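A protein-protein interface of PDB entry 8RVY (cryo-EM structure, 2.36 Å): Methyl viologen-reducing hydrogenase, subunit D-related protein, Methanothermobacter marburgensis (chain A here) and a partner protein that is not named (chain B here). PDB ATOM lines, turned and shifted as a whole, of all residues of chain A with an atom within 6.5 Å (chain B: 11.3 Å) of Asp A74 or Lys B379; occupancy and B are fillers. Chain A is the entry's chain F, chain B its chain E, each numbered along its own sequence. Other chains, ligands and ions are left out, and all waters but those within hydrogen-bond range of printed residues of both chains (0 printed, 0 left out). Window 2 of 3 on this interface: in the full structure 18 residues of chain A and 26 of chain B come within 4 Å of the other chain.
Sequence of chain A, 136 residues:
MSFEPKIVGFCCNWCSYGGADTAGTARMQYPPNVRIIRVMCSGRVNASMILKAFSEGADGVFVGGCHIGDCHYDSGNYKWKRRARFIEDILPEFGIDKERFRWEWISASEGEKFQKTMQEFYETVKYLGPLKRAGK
The guanidinium group of Arg A82 is in hydrogen-bond range of the backbone carbonyl oxygen of Met B374 (3.2 Å). The backbone carbonyl oxygen (O) of Ser B376 is in hydrogen-bond range of the guanidinium group (NH1) of Arg A82. O of Glu B378 lies within hydrogen-bond range of NH2 of Arg A82 (2.8 Å). OD1 of Asp A74 lies within salt-bridge range of NZ of Lys B379, at 3.2 Å.
OG of Ser B376 is in hydrogen-bond range of N of Glu B378, 3.2 Å away. OD1 of Asp B380 is in hydrogen-bond range of OG of Ser B376, 2.6 Å away. The backbone NH (N) of Asp A74 lies close to the side-chain sulfur (SG) of Cys A71, 3.6 Å away. The side-chain hydroxyl (OG) of Ser A75 lies within hydrogen-bond range of the side-chain amino group (NZ) of Lys A79, 3.3 Å away.
Among the printed residues, pairs that only touch across the chains: Tyr A78 with Lys B379, Lys A79 with Ser B376, Arg A82 with Pro B373 and Arg A82 with Asp B380.
No residue of chain B comes within 4 Å of Cys A71. His A72 touches none of the printed residues of chain B. Of chain B, only Lys B379 (3.2 Å) comes within 4 Å of Asp A74. No residue of chain B comes within 4 Å of Ser A75. Of the printed residues of chain B, Lys A79 touches Ser B376 (3.99 Å). Printed residues of chain B within 4 Å of Arg A82: Pro B373 (3.4 Å), Met B374 (3.2 Å), Ser B376 (2.6 Å), Glu B378 (2.8 Å) and Asp B380 (3.6 Å). Printed residues of chain A within 4 Å of Met B374: Arg A82 (3.2 Å). Printed residues of chain A within 4 Å of Ser B376: Lys A79 and Arg A82. The nearest residue of chain B that does not touch Asp A74 is Gly B377 (7.7 Å). The nearest printed residue of chain B that does not touch Arg A82 is Tyr B375 (4.3 Å).
Of the 8 printed residues of chain B, 6 touch a printed residue of chain A. Among the printed residues, 8 pairs touch across the chains. Among the printed residues, Asp or Glu carboxylates within 4 Å of a Lys or Arg side-chain nitrogen of the other chain: Asp A74 with Lys B379 (3.2 Å).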
ATOM      1  N   CYS A  41     -20.370   3.304 -30.489  1.00  0.00           N
ATOM      2  CA  CYS A  41     -19.964   2.010 -31.008  1.00  0.00           C
ATOM      3  C   CYS A  41     -21.143   1.059 -30.918  1.00  0.00           C
ATOM      4  O   CYS A  41     -22.025   1.224 -30.075  1.00  0.00           O
ATOM      5  CB  CYS A  41     -18.768   1.457 -30.222  1.00  0.00           C
ATOM      6  SG  CYS A  41     -18.095  -0.099 -30.821  1.00  0.00           S
ATOM      7  N   GLY A  69     -13.170  -5.901 -37.766  1.00  0.00           N
ATOM      8  CA  GLY A  69     -11.832  -5.417 -38.002  1.00  0.00           C
ATOM      9  C   GLY A  69     -11.734  -3.917 -38.192  1.00  0.00           C
ATOM     10  O   GLY A  69     -10.629  -3.372 -38.121  1.00  0.00           O
ATOM     11  N   ASP A  70     -12.857  -3.239 -38.424  1.00  0.00           N
ATOM     12  CA  ASP A  70     -12.877  -1.806 -38.681  1.00  0.00           C
ATOM     13  C   ASP A  70     -13.325  -0.985 -37.480  1.00  0.00           C
ATOM     14  O   ASP A  70     -13.382   0.243 -37.580  1.00  0.00           O
ATOM     15  CB  ASP A  70     -13.799  -1.499 -39.864  1.00  0.00           C
ATOM     16  CG  ASP A  70     -13.149  -1.781 -41.200  1.00  0.00           C
ATOM     17  OD1 ASP A  70     -12.131  -2.500 -41.229  1.00  0.00           O
ATOM     18  OD2 ASP A  70     -13.663  -1.290 -42.226  1.00  0.00           O
ATOM     19  N   CYS A  71     -13.638  -1.621 -36.354  1.00  0.00           N
ATOM     20  CA  CYS A  71     -14.201  -0.901 -35.220  1.00  0.00           C
ATOM     21  C   CYS A  71     -13.263   0.204 -34.761  1.00  0.00           C
ATOM     22  O   CYS A  71     -12.064  -0.011 -34.575  1.00  0.00           O
ATOM     23  CB  CYS A  71     -14.474  -1.867 -34.067  1.00  0.00           C
ATOM     24  SG  CYS A  71     -15.197  -1.121 -32.596  1.00  0.00           S
ATOM     25  N   HIS A  72     -13.824   1.396 -34.563  1.00  0.00           N
ATOM     26  CA  HIS A  72     -13.048   2.534 -34.097  1.00  0.00           C
ATOM     27  C   HIS A  72     -12.502   2.330 -32.693  1.00  0.00           C
ATOM     28  O   HIS A  72     -11.577   3.044 -32.296  1.00  0.00           O
ATOM     29  CB  HIS A  72     -13.912   3.792 -34.149  1.00  0.00           C
ATOM     30  CG  HIS A  72     -13.179   5.049 -33.804  1.00  0.00           C
ATOM     31  ND1 HIS A  72     -12.953   5.447 -32.504  1.00  0.00           N
ATOM     32  CD2 HIS A  72     -12.628   6.002 -34.589  1.00  0.00           C
ATOM     33  CE1 HIS A  72     -12.292   6.590 -32.505  1.00  0.00           C
ATOM     34  NE2 HIS A  72     -12.081   6.947 -33.757  1.00  0.00           N
ATOM     35  N   TYR A  73     -13.050   1.376 -31.939  1.00  0.00           N
ATOM     36  CA  TYR A  73     -12.578   1.050 -30.598  1.00  0.00           C
ATOM     37  C   TYR A  73     -11.995  -0.358 -30.546  1.00  0.00           C
ATOM     38  O   TYR A  73     -11.777  -0.906 -29.463  1.00  0.00           O
ATOM     39  CB  TYR A  73     -13.722   1.226 -29.603  1.00  0.00           C
ATOM     40  CG  TYR A  73     -14.286   2.626 -29.640  1.00  0.00           C
ATOM     41  CD1 TYR A  73     -13.645   3.671 -28.992  1.00  0.00           C
ATOM     42  CD2 TYR A  73     -15.444   2.907 -30.347  1.00  0.00           C
ATOM     43  CE1 TYR A  73     -14.151   4.949 -29.035  1.00  0.00           C
ATOM     44  CE2 TYR A  73     -15.954   4.181 -30.395  1.00  0.00           C
ATOM     45  CZ  TYR A  73     -15.304   5.198 -29.739  1.00  0.00           C
ATOM     46  OH  TYR A  73     -15.813   6.471 -29.784  1.00  0.00           O
ATOM     47  N   ASP A  74     -11.762  -0.946 -31.715  1.00  0.00           N
ATOM     48  CA  ASP A  74     -10.934  -2.125 -31.933  1.00  0.00           C
ATOM     49  C   ASP A  74     -11.551  -3.470 -31.569  1.00  0.00           C
ATOM     50  O   ASP A  74     -11.067  -4.496 -32.052  1.00  0.00           O
ATOM     51  CB  ASP A  74      -9.638  -1.972 -31.130  1.00  0.00           C
ATOM     52  CG  ASP A  74      -8.665  -3.107 -31.362  1.00  0.00           C
ATOM     53  OD1 ASP A  74      -8.110  -3.203 -32.476  1.00  0.00           O
ATOM     54  OD2 ASP A  74      -8.459  -3.908 -30.428  1.00  0.00           O
ATOM     55  N   SER A  75     -12.616  -3.515 -30.769  1.00  0.00           N
ATOM     56  CA  SER A  75     -13.263  -4.796 -30.506  1.00  0.00           C
ATOM     57  C   SER A  75     -14.754  -4.702 -30.203  1.00  0.00           C
ATOM     58  O   SER A  75     -15.372  -5.730 -29.914  1.00  0.00           O
ATOM     59  CB  SER A  75     -12.545  -5.523 -29.363  1.00  0.00           C
ATOM     60  OG  SER A  75     -12.005  -4.614 -28.428  1.00  0.00           O
ATOM     61  N   GLY A  76     -15.354  -3.514 -30.256  1.00  0.00           N
ATOM     62  CA  GLY A  76     -16.724  -3.376 -29.790  1.00  0.00           C
ATOM     63  C   GLY A  76     -17.707  -4.206 -30.592  1.00  0.00           C
ATOM     64  O   GLY A  76     -18.628  -4.813 -30.034  1.00  0.00           O
ATOM     65  N   ASN A  77     -17.524  -4.248 -31.911  1.00  0.00           N
ATOM     66  CA  ASN A  77     -18.461  -4.977 -32.755  1.00  0.00           C
ATOM     67  C   ASN A  77     -18.388  -6.480 -32.509  1.00  0.00           C
ATOM     68  O   ASN A  77     -19.342  -7.200 -32.799  1.00  0.00           O
ATOM     69  CB  ASN A  77     -18.219  -4.645 -34.230  1.00  0.00           C
ATOM     70  CG  ASN A  77     -16.758  -4.658 -34.611  1.00  0.00           C
ATOM     71  OD1 ASN A  77     -15.888  -4.901 -33.783  1.00  0.00           O
ATOM     72  ND2 ASN A  77     -16.481  -4.375 -35.871  1.00  0.00           N
ATOM     73  N   TYR A  78     -17.286  -6.970 -31.938  1.00  0.00           N
ATOM     74  CA  TYR A  78     -17.215  -8.384 -31.572  1.00  0.00           C
ATOM     75  C   TYR A  78     -18.170  -8.708 -30.428  1.00  0.00           C
ATOM     76  O   TYR A  78     -18.943  -9.676 -30.496  1.00  0.00           O
ATOM     77  CB  TYR A  78     -15.786  -8.747 -31.178  1.00  0.00           C
ATOM     78  CG  TYR A  78     -14.835  -8.892 -32.338  1.00  0.00           C
ATOM     79  CD1 TYR A  78     -14.723 -10.091 -33.022  1.00  0.00           C
ATOM     80  CD2 TYR A  78     -14.042  -7.832 -32.742  1.00  0.00           C
ATOM     81  CE1 TYR A  78     -13.853 -10.228 -34.077  1.00  0.00           C
ATOM     82  CE2 TYR A  78     -13.171  -7.958 -33.797  1.00  0.00           C
ATOM     83  CZ  TYR A  78     -13.078  -9.159 -34.460  1.00  0.00           C
ATOM     84  OH  TYR A  78     -12.208  -9.289 -35.513  1.00  0.00           O
ATOM     85  N   LYS A  79     -18.123  -7.906 -29.365  1.00  0.00           N
ATOM     86  CA  LYS A  79     -19.076  -8.062 -28.275  1.00  0.00           C
ATOM     87  C   LYS A  79     -20.499  -7.897 -28.780  1.00  0.00           C
ATOM     88  O   LYS A  79     -21.397  -8.660 -28.396  1.00  0.00           O
ATOM     89  CB  LYS A  79     -18.778  -7.046 -27.177  1.00  0.00           C
ATOM     90  CG  LYS A  79     -17.594  -7.403 -26.305  1.00  0.00           C
ATOM     91  CD  LYS A  79     -16.281  -6.993 -26.938  1.00  0.00           C
ATOM     92  CE  LYS A  79     -15.135  -7.161 -25.960  1.00  0.00           C
ATOM     93  NZ  LYS A  79     -13.871  -6.557 -26.454  1.00  0.00           N
ATOM     94  N   LYS A  81     -21.617  -8.544 -31.769  1.00  0.00           N
ATOM     95  CA  LYS A  81     -21.986  -9.717 -32.556  1.00  0.00           C
ATOM     96  C   LYS A  81     -22.369 -10.883 -31.655  1.00  0.00           C
ATOM     97  O   LYS A  81     -23.346 -11.596 -31.925  1.00  0.00           O
ATOM     98  CB  LYS A  81     -20.831 -10.105 -33.477  1.00  0.00           C
ATOM     99  CG  LYS A  81     -21.118 -11.296 -34.362  1.00  0.00           C
ATOM    100  CD  LYS A  81     -20.117 -11.398 -35.494  1.00  0.00           C
ATOM    101  CE  LYS A  81     -18.695 -11.469 -34.973  1.00  0.00           C
ATOM    102  NZ  LYS A  81     -17.779 -12.128 -35.942  1.00  0.00           N
ATOM    103  N   ARG A  82     -21.605 -11.099 -30.584  1.00  0.00           N
ATOM    104  CA  ARG A  82     -21.994 -12.115 -29.610  1.00  0.00           C
ATOM    105  C   ARG A  82     -23.400 -11.849 -29.085  1.00  0.00           C
ATOM    106  O   ARG A  82     -24.269 -12.739 -29.088  1.00  0.00           O
ATOM    107  CB  ARG A  82     -20.999 -12.138 -28.454  1.00  0.00           C
ATOM    108  CG  ARG A  82     -19.686 -12.794 -28.776  1.00  0.00           C
ATOM    109  CD  ARG A  82     -18.701 -12.595 -27.650  1.00  0.00           C
ATOM    110  NE  ARG A  82     -17.361 -12.320 -28.152  1.00  0.00           N
ATOM    111  CZ  ARG A  82     -16.421 -11.680 -27.472  1.00  0.00           C
ATOM    112  NH1 ARG A  82     -16.640 -11.221 -26.252  1.00  0.00           N
ATOM    113  NH2 ARG A  82     -15.229 -11.500 -28.032  1.00  0.00           N
ATOM    114  N   PRO B 373     -18.368 -17.519 -23.187  1.00  0.00           N
ATOM    115  CA  PRO B 373     -17.693 -16.777 -24.264  1.00  0.00           C
ATOM    116  C   PRO B 373     -18.251 -15.380 -24.471  1.00  0.00           C
ATOM    117  O   PRO B 373     -17.554 -14.532 -25.036  1.00  0.00           O
ATOM    118  CB  PRO B 373     -17.914 -17.656 -25.502  1.00  0.00           C
ATOM    119  CG  PRO B 373     -18.327 -18.979 -25.006  1.00  0.00           C
ATOM    120  CD  PRO B 373     -18.848 -18.841 -23.619  1.00  0.00           C
ATOM    121  N   MET B 374     -19.484 -15.117 -24.034  1.00  0.00           N
ATOM    122  CA  MET B 374     -20.053 -13.777 -24.138  1.00  0.00           C
ATOM    123  C   MET B 374     -19.120 -12.728 -23.546  1.00  0.00           C
ATOM    124  O   MET B 374     -18.966 -11.637 -24.104  1.00  0.00           O
ATOM    125  CB  MET B 374     -21.412 -13.740 -23.433  1.00  0.00           C
ATOM    126  CG  MET B 374     -22.121 -12.388 -23.470  1.00  0.00           C
ATOM    127  SD  MET B 374     -22.923 -11.980 -25.035  1.00  0.00           S
ATOM    128  CE  MET B 374     -23.849 -13.467 -25.378  1.00  0.00           C
ATOM    129  N   TYR B 375     -18.492 -13.036 -22.410  1.00  0.00           N
ATOM    130  CA  TYR B 375     -17.602 -12.106 -21.727  1.00  0.00           C
ATOM    131  C   TYR B 375     -16.145 -12.295 -22.118  1.00  0.00           C
ATOM    132  O   TYR B 375     -15.249 -11.992 -21.320  1.00  0.00           O
ATOM    133  CB  TYR B 375     -17.761 -12.249 -20.214  1.00  0.00           C
ATOM    134  CG  TYR B 375     -19.178 -12.078 -19.733  1.00  0.00           C
ATOM    135  CD1 TYR B 375     -19.959 -11.024 -20.180  1.00  0.00           C
ATOM    136  CD2 TYR B 375     -19.732 -12.966 -18.827  1.00  0.00           C
ATOM    137  CE1 TYR B 375     -21.252 -10.864 -19.740  1.00  0.00           C
ATOM    138  CE2 TYR B 375     -21.022 -12.813 -18.382  1.00  0.00           C
ATOM    139  CZ  TYR B 375     -21.779 -11.762 -18.843  1.00  0.00           C
ATOM    140  OH  TYR B 375     -23.070 -11.605 -18.399  1.00  0.00           O
ATOM    141  N   SER B 376     -15.883 -12.792 -23.321  1.00  0.00           N
ATOM    142  CA  SER B 376     -14.519 -13.044 -23.760  1.00  0.00           C
ATOM    143  C   SER B 376     -13.853 -11.746 -24.197  1.00  0.00           C
ATOM    144  O   SER B 376     -14.439 -10.956 -24.942  1.00  0.00           O
ATOM    145  CB  SER B 376     -14.513 -14.052 -24.907  1.00  0.00           C
ATOM    146  OG  SER B 376     -13.247 -14.094 -25.534  1.00  0.00           O
ATOM    147  N   GLY B 377     -12.630 -11.529 -23.729  1.00  0.00           N
ATOM    148  CA  GLY B 377     -11.833 -10.396 -24.136  1.00  0.00           C
ATOM    149  C   GLY B 377     -10.973 -10.629 -25.353  1.00  0.00           C
ATOM    150  O   GLY B 377     -10.199  -9.745 -25.730  1.00  0.00           O
ATOM    151  N   GLU B 378     -11.078 -11.794 -25.982  1.00  0.00           N
ATOM    152  CA  GLU B 378     -10.324 -12.098 -27.185  1.00  0.00           C
ATOM    153  C   GLU B 378     -11.296 -11.688 -28.286  1.00  0.00           C
ATOM    154  O   GLU B 378     -12.464 -11.383 -28.041  1.00  0.00           O
ATOM    155  CB  GLU B 378      -9.919 -13.573 -27.211  1.00  0.00           C
ATOM    156  CG  GLU B 378      -9.371 -14.103 -25.895  1.00  0.00           C
ATOM    157  CD  GLU B 378      -8.101 -13.401 -25.460  1.00  0.00           C
ATOM    158  OE1 GLU B 378      -7.568 -12.587 -26.240  1.00  0.00           O
ATOM    159  OE2 GLU B 378      -7.633 -13.665 -24.332  1.00  0.00           O
ATOM    160  N   LYS B 379     -10.796 -11.685 -29.519  1.00  0.00           N
ATOM    161  CA  LYS B 379     -11.608 -11.343 -30.680  1.00  0.00           C
ATOM    162  C   LYS B 379     -12.085 -12.623 -31.486  1.00  0.00           C
ATOM    163  O   LYS B 379     -12.200 -12.702 -32.714  1.00  0.00           O
ATOM    164  CB  LYS B 379     -10.768 -10.562 -31.689  1.00  0.00           C
ATOM    165  CG  LYS B 379     -10.341  -9.184 -31.219  1.00  0.00           C
ATOM    166  CD  LYS B 379      -9.493  -8.481 -32.261  1.00  0.00           C
ATOM    167  CE  LYS B 379      -9.089  -7.098 -31.800  1.00  0.00           C
ATOM    168  NZ  LYS B 379      -8.237  -6.394 -32.791  1.00  0.00           N
ATOM    169  N   ASP B 380     -12.341 -13.648 -30.683  1.00  0.00           N
ATOM    170  CA  ASP B 380     -12.868 -14.903 -31.196  1.00  0.00           C
ATOM    171  C   ASP B 380     -14.269 -14.453 -31.588  1.00  0.00           C
ATOM    172  O   ASP B 380     -14.853 -13.584 -30.942  1.00  0.00           O
ATOM    173  CB  ASP B 380     -12.943 -16.007 -30.136  1.00  0.00           C
ATOM    174  CG  ASP B 380     -13.580 -15.534 -28.843  1.00  0.00           C
ATOM    175  OD1 ASP B 380     -12.846 -15.038 -27.965  1.00  0.00           O
ATOM    176  OD2 ASP B 380     -14.815 -15.657 -28.704  1.00  0.00           O
